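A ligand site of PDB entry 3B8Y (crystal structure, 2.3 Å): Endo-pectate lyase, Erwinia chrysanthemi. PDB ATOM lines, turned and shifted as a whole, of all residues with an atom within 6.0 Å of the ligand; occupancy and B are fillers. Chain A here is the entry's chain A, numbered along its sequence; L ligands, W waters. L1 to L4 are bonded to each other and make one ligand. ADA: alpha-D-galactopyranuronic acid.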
ATOM      1  N   SER A 147      28.958  -7.578  13.630  1.00  0.00           N
ATOM      2  CA  SER A 147      29.227  -7.893  12.225  1.00  0.00           C
ATOM      3  C   SER A 147      28.742  -9.282  11.795  1.00  0.00           C
ATOM      4  O   SER A 147      29.539 -10.161  11.457  1.00  0.00           O
ATOM      5  CB  SER A 147      30.711  -7.712  11.922  1.00  0.00           C
ATOM      6  OG  SER A 147      30.963  -7.820  10.521  1.00  0.00           O
ATOM      7  N   ASP A 173      30.054 -19.366  13.847  1.00  0.00           N
ATOM      8  CA  ASP A 173      29.437 -19.492  12.524  1.00  0.00           C
ATOM      9  C   ASP A 173      29.348 -20.944  12.028  1.00  0.00           C
ATOM     10  O   ASP A 173      29.427 -21.208  10.827  1.00  0.00           O
ATOM     11  CB  ASP A 173      30.119 -18.591  11.492  1.00  0.00           C
ATOM     12  CG  ASP A 173      29.197 -18.285  10.303  1.00  0.00           C
ATOM     13  OD1 ASP A 173      29.699 -18.152   9.166  1.00  0.00           O
ATOM     14  OD2 ASP A 173      27.975 -18.186  10.507  1.00  0.00           O
ATOM     15  N   ASP A 195      25.111 -19.281  11.477  1.00  0.00           N
ATOM     16  CA  ASP A 195      24.763 -20.253  10.441  1.00  0.00           C
ATOM     17  C   ASP A 195      25.152 -21.613  11.019  1.00  0.00           C
ATOM     18  O   ASP A 195      26.135 -21.708  11.757  1.00  0.00           O
ATOM     19  CB  ASP A 195      25.562 -19.992   9.163  1.00  0.00           C
ATOM     20  CG  ASP A 195      25.183 -18.676   8.470  1.00  0.00           C
ATOM     21  OD1 ASP A 195      24.120 -18.085   8.775  1.00  0.00           O
ATOM     22  OD2 ASP A 195      25.972 -18.235   7.597  1.00  0.00           O
ATOM     23  N   THR A 198      27.691 -23.905   6.344  1.00  0.00           N
ATOM     24  CA  THR A 198      27.799 -23.080   5.154  1.00  0.00           C
ATOM     25  C   THR A 198      28.503 -23.839   4.045  1.00  0.00           C
ATOM     26  O   THR A 198      29.558 -24.433   4.249  1.00  0.00           O
ATOM     27  CB  THR A 198      28.550 -21.752   5.476  1.00  0.00           C
ATOM     28  OG1 THR A 198      27.821 -21.013   6.464  1.00  0.00           O
ATOM     29  CG2 THR A 198      28.697 -20.881   4.245  1.00  0.00           C
ATOM     30  N   LYS A 224      19.518 -18.938  10.150  1.00  0.00           N
ATOM     31  CA  LYS A 224      19.815 -19.657   8.917  1.00  0.00           C
ATOM     32  C   LYS A 224      20.416 -20.991   9.305  1.00  0.00           C
ATOM     33  O   LYS A 224      21.363 -21.033  10.099  1.00  0.00           O
ATOM     34  CB  LYS A 224      20.851 -18.884   8.100  1.00  0.00           C
ATOM     35  CG  LYS A 224      20.579 -18.809   6.609  1.00  0.00           C
ATOM     36  CD  LYS A 224      19.788 -17.553   6.298  1.00  0.00           C
ATOM     37  CE  LYS A 224      20.484 -16.326   6.854  1.00  0.00           C
ATOM     38  NZ  LYS A 224      19.640 -15.094   6.722  1.00  0.00           N
ATOM     39  N   GLN A 227      23.395 -22.424   4.829  1.00  0.00           N
ATOM     40  CA  GLN A 227      23.708 -21.270   3.986  1.00  0.00           C
ATOM     41  C   GLN A 227      24.534 -21.755   2.812  1.00  0.00           C
ATOM     42  O   GLN A 227      25.553 -22.431   2.999  1.00  0.00           O
ATOM     43  CB  GLN A 227      24.542 -20.255   4.778  1.00  0.00           C
ATOM     44  CG  GLN A 227      23.862 -18.917   5.009  1.00  0.00           C
ATOM     45  CD  GLN A 227      23.526 -18.184   3.732  1.00  0.00           C
ATOM     46  OE1 GLN A 227      24.387 -17.959   2.883  1.00  0.00           O
ATOM     47  NE2 GLN A 227      22.263 -17.802   3.588  1.00  0.00           N
ATOM     48  N   HIS A 228      24.101 -21.425   1.602  1.00  0.00           N
ATOM     49  CA  HIS A 228      24.786 -21.851   0.376  1.00  0.00           C
ATOM     50  C   HIS A 228      25.324 -20.625  -0.350  1.00  0.00           C
ATOM     51  O   HIS A 228      24.549 -19.834  -0.888  1.00  0.00           O
ATOM     52  CB  HIS A 228      23.765 -22.570  -0.510  1.00  0.00           C
ATOM     53  CG  HIS A 228      24.366 -23.541  -1.475  1.00  0.00           C
ATOM     54  ND1 HIS A 228      23.785 -24.759  -1.756  1.00  0.00           N
ATOM     55  CD2 HIS A 228      25.439 -23.444  -2.299  1.00  0.00           C
ATOM     56  CE1 HIS A 228      24.462 -25.359  -2.709  1.00  0.00           C
ATOM     57  NE2 HIS A 228      25.472 -24.587  -3.055  1.00  0.00           N
ATOM     58  N   ASN A 229      26.649 -20.467  -0.370  1.00  0.00           N
ATOM     59  CA  ASN A 229      27.287 -19.311  -1.011  1.00  0.00           C
ATOM     60  C   ASN A 229      28.067 -19.638  -2.285  1.00  0.00           C
ATOM     61  O   ASN A 229      28.239 -18.786  -3.147  1.00  0.00           O
ATOM     62  CB  ASN A 229      28.199 -18.584  -0.028  1.00  0.00           C
ATOM     63  CG  ASN A 229      27.477 -18.105   1.207  1.00  0.00           C
ATOM     64  OD1 ASN A 229      26.312 -17.744   1.158  1.00  0.00           O
ATOM     65  ND2 ASN A 229      28.170 -18.141   2.336  1.00  0.00           N
ATOM     66  N   LYS A 249      15.096 -20.199   7.878  1.00  0.00           N
ATOM     67  CA  LYS A 249      15.019 -21.076   6.719  1.00  0.00           C
ATOM     68  C   LYS A 249      15.904 -22.296   6.941  1.00  0.00           C
ATOM     69  O   LYS A 249      16.899 -22.229   7.653  1.00  0.00           O
ATOM     70  CB  LYS A 249      15.441 -20.351   5.437  1.00  0.00           C
ATOM     71  CG  LYS A 249      14.506 -19.222   5.026  1.00  0.00           C
ATOM     72  CD  LYS A 249      14.967 -18.542   3.740  1.00  0.00           C
ATOM     73  CE  LYS A 249      14.166 -17.286   3.434  1.00  0.00           C
ATOM     74  NZ  LYS A 249      14.347 -16.233   4.455  1.00  0.00           N
ATOM     75  N   ARG A 252      18.982 -21.668   2.308  1.00  0.00           N
ATOM     76  CA  ARG A 252      18.879 -20.435   1.557  1.00  0.00           C
ATOM     77  C   ARG A 252      20.073 -20.220   0.618  1.00  0.00           C
ATOM     78  O   ARG A 252      21.224 -20.208   1.056  1.00  0.00           O
ATOM     79  CB  ARG A 252      18.786 -19.244   2.512  1.00  0.00           C
ATOM     80  CG  ARG A 252      18.705 -17.912   1.816  1.00  0.00           C
ATOM     81  CD  ARG A 252      17.557 -17.879   0.825  1.00  0.00           C
ATOM     82  NE  ARG A 252      17.169 -16.502   0.558  1.00  0.00           N
ATOM     83  CZ  ARG A 252      17.225 -15.908  -0.637  1.00  0.00           C
ATOM     84  NH1 ARG A 252      16.855 -14.636  -0.752  1.00  0.00           N
ATOM     85  NH2 ARG A 252      17.609 -16.603  -1.707  1.00  0.00           N
ATOM     86  N   SER A 253      19.774 -20.112  -0.674  1.00  0.00           N
ATOM     87  CA  SER A 253      20.814 -19.802  -1.650  1.00  0.00           C
ATOM     88  C   SER A 253      21.003 -18.310  -1.424  1.00  0.00           C
ATOM     89  O   SER A 253      20.066 -17.533  -1.593  1.00  0.00           O
ATOM     90  CB  SER A 253      20.293 -20.007  -3.065  1.00  0.00           C
ATOM     91  OG  SER A 253      21.208 -19.446  -3.993  1.00  0.00           O
ATOM     92  N   CYS A 254      22.203 -17.919  -0.985  1.00  0.00           N
ATOM     93  CA  CYS A 254      22.505 -16.533  -0.689  1.00  0.00           C
ATOM     94  C   CYS A 254      21.817 -15.539  -1.621  1.00  0.00           C
ATOM     95  O   CYS A 254      21.968 -15.603  -2.843  1.00  0.00           O
ATOM     96  CB  CYS A 254      24.005 -16.294  -0.702  1.00  0.00           C
ATOM     97  SG  CYS A 254      24.406 -14.712   0.066  1.00  0.00           S
ATOM     98  N   GLY A 255      21.044 -14.638  -1.021  1.00  0.00           N
ATOM     99  CA  GLY A 255      20.306 -13.646  -1.798  1.00  0.00           C
ATOM    100  C   GLY A 255      21.071 -12.389  -2.176  1.00  0.00           C
ATOM    101  O   GLY A 255      20.841 -11.853  -3.264  1.00  0.00           O
ATOM    102  N   ASP A 256      21.984 -11.940  -1.316  1.00  0.00           N
ATOM    103  CA  ASP A 256      22.725 -10.709  -1.575  1.00  0.00           C
ATOM    104  C   ASP A 256      24.237 -10.795  -1.367  1.00  0.00           C
ATOM    105  O   ASP A 256      24.863  -9.827  -0.949  1.00  0.00           O
ATOM    106  CB  ASP A 256      22.155  -9.571  -0.714  1.00  0.00           C
ATOM    107  CG  ASP A 256      22.256  -9.855   0.798  1.00  0.00           C
ATOM    108  OD1 ASP A 256      21.643  -9.097   1.577  1.00  0.00           O
ATOM    109  OD2 ASP A 256      22.918 -10.824   1.213  1.00  0.00           O
ATOM    110  N   CYS A 257      24.831 -11.943  -1.648  1.00  0.00           N
ATOM    111  CA  CYS A 257      26.267 -12.124  -1.470  1.00  0.00           C
ATOM    112  C   CYS A 257      27.129 -11.283  -2.391  1.00  0.00           C
ATOM    113  O   CYS A 257      26.679 -10.902  -3.476  1.00  0.00           O
ATOM    114  CB  CYS A 257      26.646 -13.582  -1.644  1.00  0.00           C
ATOM    115  SG  CYS A 257      26.418 -14.567  -0.137  1.00  0.00           S
ATOM    116  N   SER A 258      28.347 -10.978  -1.947  1.00  0.00           N
ATOM    117  CA  SER A 258      29.292 -10.228  -2.768  1.00  0.00           C
ATOM    118  C   SER A 258      29.702 -11.215  -3.833  1.00  0.00           C
ATOM    119  O   SER A 258      30.078 -12.357  -3.532  1.00  0.00           O
ATOM    120  CB  SER A 258      30.500  -9.798  -1.936  1.00  0.00           C
ATOM    121  OG  SER A 258      30.125  -8.835  -0.957  1.00  0.00           O
ATOM    122  N   ASN A 259      29.604 -10.802  -5.094  1.00  0.00           N
ATOM    123  CA  ASN A 259      29.907 -11.683  -6.217  1.00  0.00           C
ATOM    124  C   ASN A 259      28.871 -12.797  -6.163  1.00  0.00           C
ATOM    125  O   ASN A 259      29.204 -13.988  -6.069  1.00  0.00           O
ATOM    126  CB  ASN A 259      31.330 -12.260  -6.103  1.00  0.00           C
ATOM    127  CG  ASN A 259      31.688 -13.188  -7.267  1.00  0.00           C
ATOM    128  OD1 ASN A 259      32.288 -14.248  -7.067  1.00  0.00           O
ATOM    129  ND2 ASN A 259      31.279 -12.811  -8.480  1.00  0.00           N
ATOM    130  N   PHE A 312      13.070 -16.151  -5.102  1.00  0.00           N
ATOM    131  CA  PHE A 312      13.508 -14.775  -4.869  1.00  0.00           C
ATOM    132  C   PHE A 312      14.256 -14.263  -6.080  1.00  0.00           C
ATOM    133  O   PHE A 312      14.552 -15.000  -7.025  1.00  0.00           O
ATOM    134  CB  PHE A 312      14.500 -14.704  -3.704  1.00  0.00           C
ATOM    135  CG  PHE A 312      13.914 -14.992  -2.368  1.00  0.00           C
ATOM    136  CD1 PHE A 312      13.621 -13.950  -1.488  1.00  0.00           C
ATOM    137  CD2 PHE A 312      13.659 -16.296  -1.976  1.00  0.00           C
ATOM    138  CE1 PHE A 312      13.089 -14.207  -0.230  1.00  0.00           C
ATOM    139  CE2 PHE A 312      13.116 -16.567  -0.714  1.00  0.00           C
ATOM    140  CZ  PHE A 312      12.830 -15.519   0.156  1.00  0.00           C
ATOM    141  N   LYS A 317      25.787  -7.883  -3.874  1.00  0.00           N
ATOM    142  CA  LYS A 317      25.916  -6.952  -2.754  1.00  0.00           C
ATOM    143  C   LYS A 317      26.105  -5.517  -3.237  1.00  0.00           C
ATOM    144  O   LYS A 317      27.006  -5.231  -4.033  1.00  0.00           O
ATOM    145  CB  LYS A 317      27.109  -7.358  -1.870  1.00  0.00           C
ATOM    146  CG  LYS A 317      27.255  -6.520  -0.627  1.00  0.00           C
ATOM    147  CD  LYS A 317      26.367  -7.009   0.492  1.00  0.00           C
ATOM    148  CE  LYS A 317      26.938  -8.268   1.114  1.00  0.00           C
ATOM    149  NZ  LYS A 317      26.036  -8.743   2.178  1.00  0.00           N
ATOM    150  N   THR A 322      17.110  -7.991  -2.266  1.00  0.00           N
ATOM    151  CA  THR A 322      16.444  -9.233  -2.680  1.00  0.00           C
ATOM    152  C   THR A 322      14.954  -9.159  -2.431  1.00  0.00           C
ATOM    153  O   THR A 322      14.518  -8.857  -1.315  1.00  0.00           O
ATOM    154  CB  THR A 322      17.016 -10.455  -1.941  1.00  0.00           C
ATOM    155  OG1 THR A 322      16.658 -10.390  -0.547  1.00  0.00           O
ATOM    156  CG2 THR A 322      18.509 -10.472  -2.050  1.00  0.00           C
HETATM  157  C1  ADA L   1      15.901 -13.071   5.950  1.00  0.00           C
HETATM  158  C2  ADA L   1      17.049 -12.097   6.208  1.00  0.00           C
HETATM  159  C3  ADA L   1      17.067 -11.059   5.102  1.00  0.00           C
HETATM  160  C4  ADA L   1      17.244 -11.785   3.753  1.00  0.00           C
HETATM  161  C5  ADA L   1      16.059 -12.756   3.606  1.00  0.00           C
HETATM  162  C6  ADA L   1      16.245 -13.482   2.299  1.00  0.00           C
HETATM  163  O1  ADA L   1      14.641 -12.390   5.982  1.00  0.00           O
HETATM  164  O2  ADA L   1      16.865 -11.449   7.458  1.00  0.00           O
HETATM  165  O3  ADA L   1      18.148 -10.145   5.319  1.00  0.00           O
HETATM  166  O4  ADA L   1      18.461 -12.569   3.715  1.00  0.00           O
HETATM  167  O5  ADA L   1      16.077 -13.711   4.681  1.00  0.00           O
HETATM  168  O6B ADA L   1      16.260 -12.807   1.147  1.00  0.00           O
HETATM  169  O6A ADA L   1      16.387 -14.682   2.317  1.00  0.00           O
HETATM  170  C1  ADA L   2      19.649 -12.024   3.190  1.00  0.00           C
HETATM  171  C2  ADA L   2      20.471 -13.085   2.456  1.00  0.00           C
HETATM  172  C3  ADA L   2      20.849 -14.179   3.426  1.00  0.00           C
HETATM  173  C4  ADA L   2      21.644 -13.556   4.554  1.00  0.00           C
HETATM  174  C5  ADA L   2      20.741 -12.489   5.231  1.00  0.00           C
HETATM  175  C6  ADA L   2      21.485 -11.855   6.390  1.00  0.00           C
HETATM  176  O2  ADA L   2      19.709 -13.653   1.393  1.00  0.00           O
HETATM  177  O3  ADA L   2      21.615 -15.165   2.751  1.00  0.00           O
HETATM  178  O4  ADA L   2      22.830 -12.946   3.992  1.00  0.00           O
HETATM  179  O5  ADA L   2      20.409 -11.462   4.278  1.00  0.00           O
HETATM  180  O6B ADA L   2      21.897 -12.618   7.406  1.00  0.00           O
HETATM  181  O6A ADA L   2      21.710 -10.665   6.406  1.00  0.00           O
HETATM  182  C1  ADA L   3      23.927 -12.595   4.812  1.00  0.00           C
HETATM  183  C2  ADA L   3      24.958 -11.771   4.023  1.00  0.00           C
HETATM  184  C3  ADA L   3      25.503 -12.648   2.922  1.00  0.00           C
HETATM  185  C4  ADA L   3      26.163 -13.870   3.565  1.00  0.00           C
HETATM  186  C5  ADA L   3      25.125 -14.614   4.398  1.00  0.00           C
HETATM  187  C6  ADA L   3      25.769 -15.799   5.073  1.00  0.00           C
HETATM  188  O2  ADA L   3      24.330 -10.636   3.440  1.00  0.00           O
HETATM  189  O3  ADA L   3      26.460 -11.926   2.157  1.00  0.00           O
HETATM  190  O4  ADA L   3      27.285 -13.505   4.390  1.00  0.00           O
HETATM  191  O5  ADA L   3      24.538 -13.750   5.410  1.00  0.00           O
HETATM  192  O6B ADA L   3      26.406 -16.735   4.349  1.00  0.00           O
HETATM  193  O6A ADA L   3      25.726 -15.898   6.289  1.00  0.00           O
HETATM  194  C1  ADA L   4      28.531 -14.011   3.987  1.00  0.00           C
HETATM  195  C2  ADA L   4      29.629 -13.827   5.051  1.00  0.00           C
HETATM  196  C3  ADA L   4      29.915 -12.335   5.225  1.00  0.00           C
HETATM  197  C4  ADA L   4      30.350 -11.775   3.878  1.00  0.00           C
HETATM  198  C5  ADA L   4      29.191 -12.004   2.880  1.00  0.00           C
HETATM  199  C6  ADA L   4      29.564 -11.432   1.539  1.00  0.00           C
HETATM  200  O2  ADA L   4      29.205 -14.404   6.283  1.00  0.00           O
HETATM  201  O3  ADA L   4      30.959 -12.156   6.197  1.00  0.00           O
HETATM  202  O4  ADA L   4      31.514 -12.467   3.423  1.00  0.00           O
HETATM  203  O5  ADA L   4      28.916 -13.425   2.718  1.00  0.00           O
HETATM  204  O6B ADA L   4      29.879 -10.136   1.422  1.00  0.00           O
HETATM  205  O6A ADA L   4      29.583 -12.151   0.565  1.00  0.00           O
HETATM  206  O   HOH W   1      28.469 -18.065   6.620  1.00  0.00           O
HETATM  207  O   HOH W   2      14.384 -10.395   8.998  1.00  0.00           O
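The side-chain sulfur of Cys 257 is in hydrogen-bond range of an oxygen (O3) of ADA L3 (3.5 Å).
The side-chain amino group (NZ) of Lys 317 sits at hydrogen-bond distance from an oxygen (O2) of ADA L3.
The side-chain carboxylate (OD2) of Asp 256 sits at hydrogen-bond distance from an oxygen (O2) of ADA L3, 2.6 Å away.
An oxygen (O6B) of ADA L4 sits at hydrogen-bond distance from the side-chain hydroxyl (OG) of Ser 258.
The side-chain hydroxyl (OG1) of Thr 322 sits at hydrogen-bond distance from an oxygen (O6B) of ADA L1 (3.0 Å).
The backbone NH (N) of Gly 255 is in hydrogen-bond range of an oxygen (O2) of ADA L2 (2.9 Å).
N of Ser 258 is in hydrogen-bond range of O6A of ADA L4 (3.0 Å).
The side-chain amino group (NZ) of Lys 224 is in salt-bridge range of an oxygen (O6B) of ADA L2.
An oxygen (O6B) of ADA L3 sits at hydrogen-bond distance from the side-chain amide nitrogen (ND2) of Asn 229 (3.0 Å).
An oxygen (O6A) of ADA L3 lies close to the side-chain carboxylate (OD2) of Asp 195, at 2.7 Å.
The side-chain amino group (NZ) of Lys 249 lies within salt-bridge range of an oxygen (O6A) of ADA L1.
The guanidinium group of Arg 252 lies within salt-bridge range of an oxygen (O6A) of ADA L1, 2.6 Å away.
OE1 of Gln 227 sits close to O6B of ADA L3 (2.8 Å).
N of His 228 is in hydrogen-bond range of O of Arg 252 (3.2 Å).
The side-chain sulfur (SG) of Cys 257 is disulfide-bonded to the side-chain sulfur (SG) of Cys 254, at 2.0 Å.
OE1 of Gln 227 lies close to OD1 of Asn 229 (2.6 Å).
The backbone NH of Lys 317 sits at hydrogen-bond distance from the backbone carbonyl oxygen of Cys 257 (3.2 Å).
The side-chain amide oxygen (OD1) of Asn 229 lies close to the side-chain sulfur (SG) of Cys 254 (3.7 Å).
The backbone carbonyl oxygen (O) of His 228 lies within hydrogen-bond range of the backbone NH (N) of Cys 254.
OD2 of Asp 173 is in hydrogen-bond range of N of Asp 195 (3.2 Å).
The side-chain amide oxygen (OD1) of Asn 229 sits close to the side-chain sulfur (SG) of Cys 257, at 3.4 Å.
Merely in contact with the ligand: Cys 254 (3.7 Å) and Phe 312 (3.7 Å).
Hydrophobic or aromatic side chains within 4 Å of the ligand: Phe 312.
The nearest printed residue that does not touch the ligand is Thr 198 (4.7 Å).
Water W1 lies within hydrogen-bond range of OD2 of Asp 195, OD1 of Asp 173, OG1 of Thr 198 and O6B of ADA L3.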
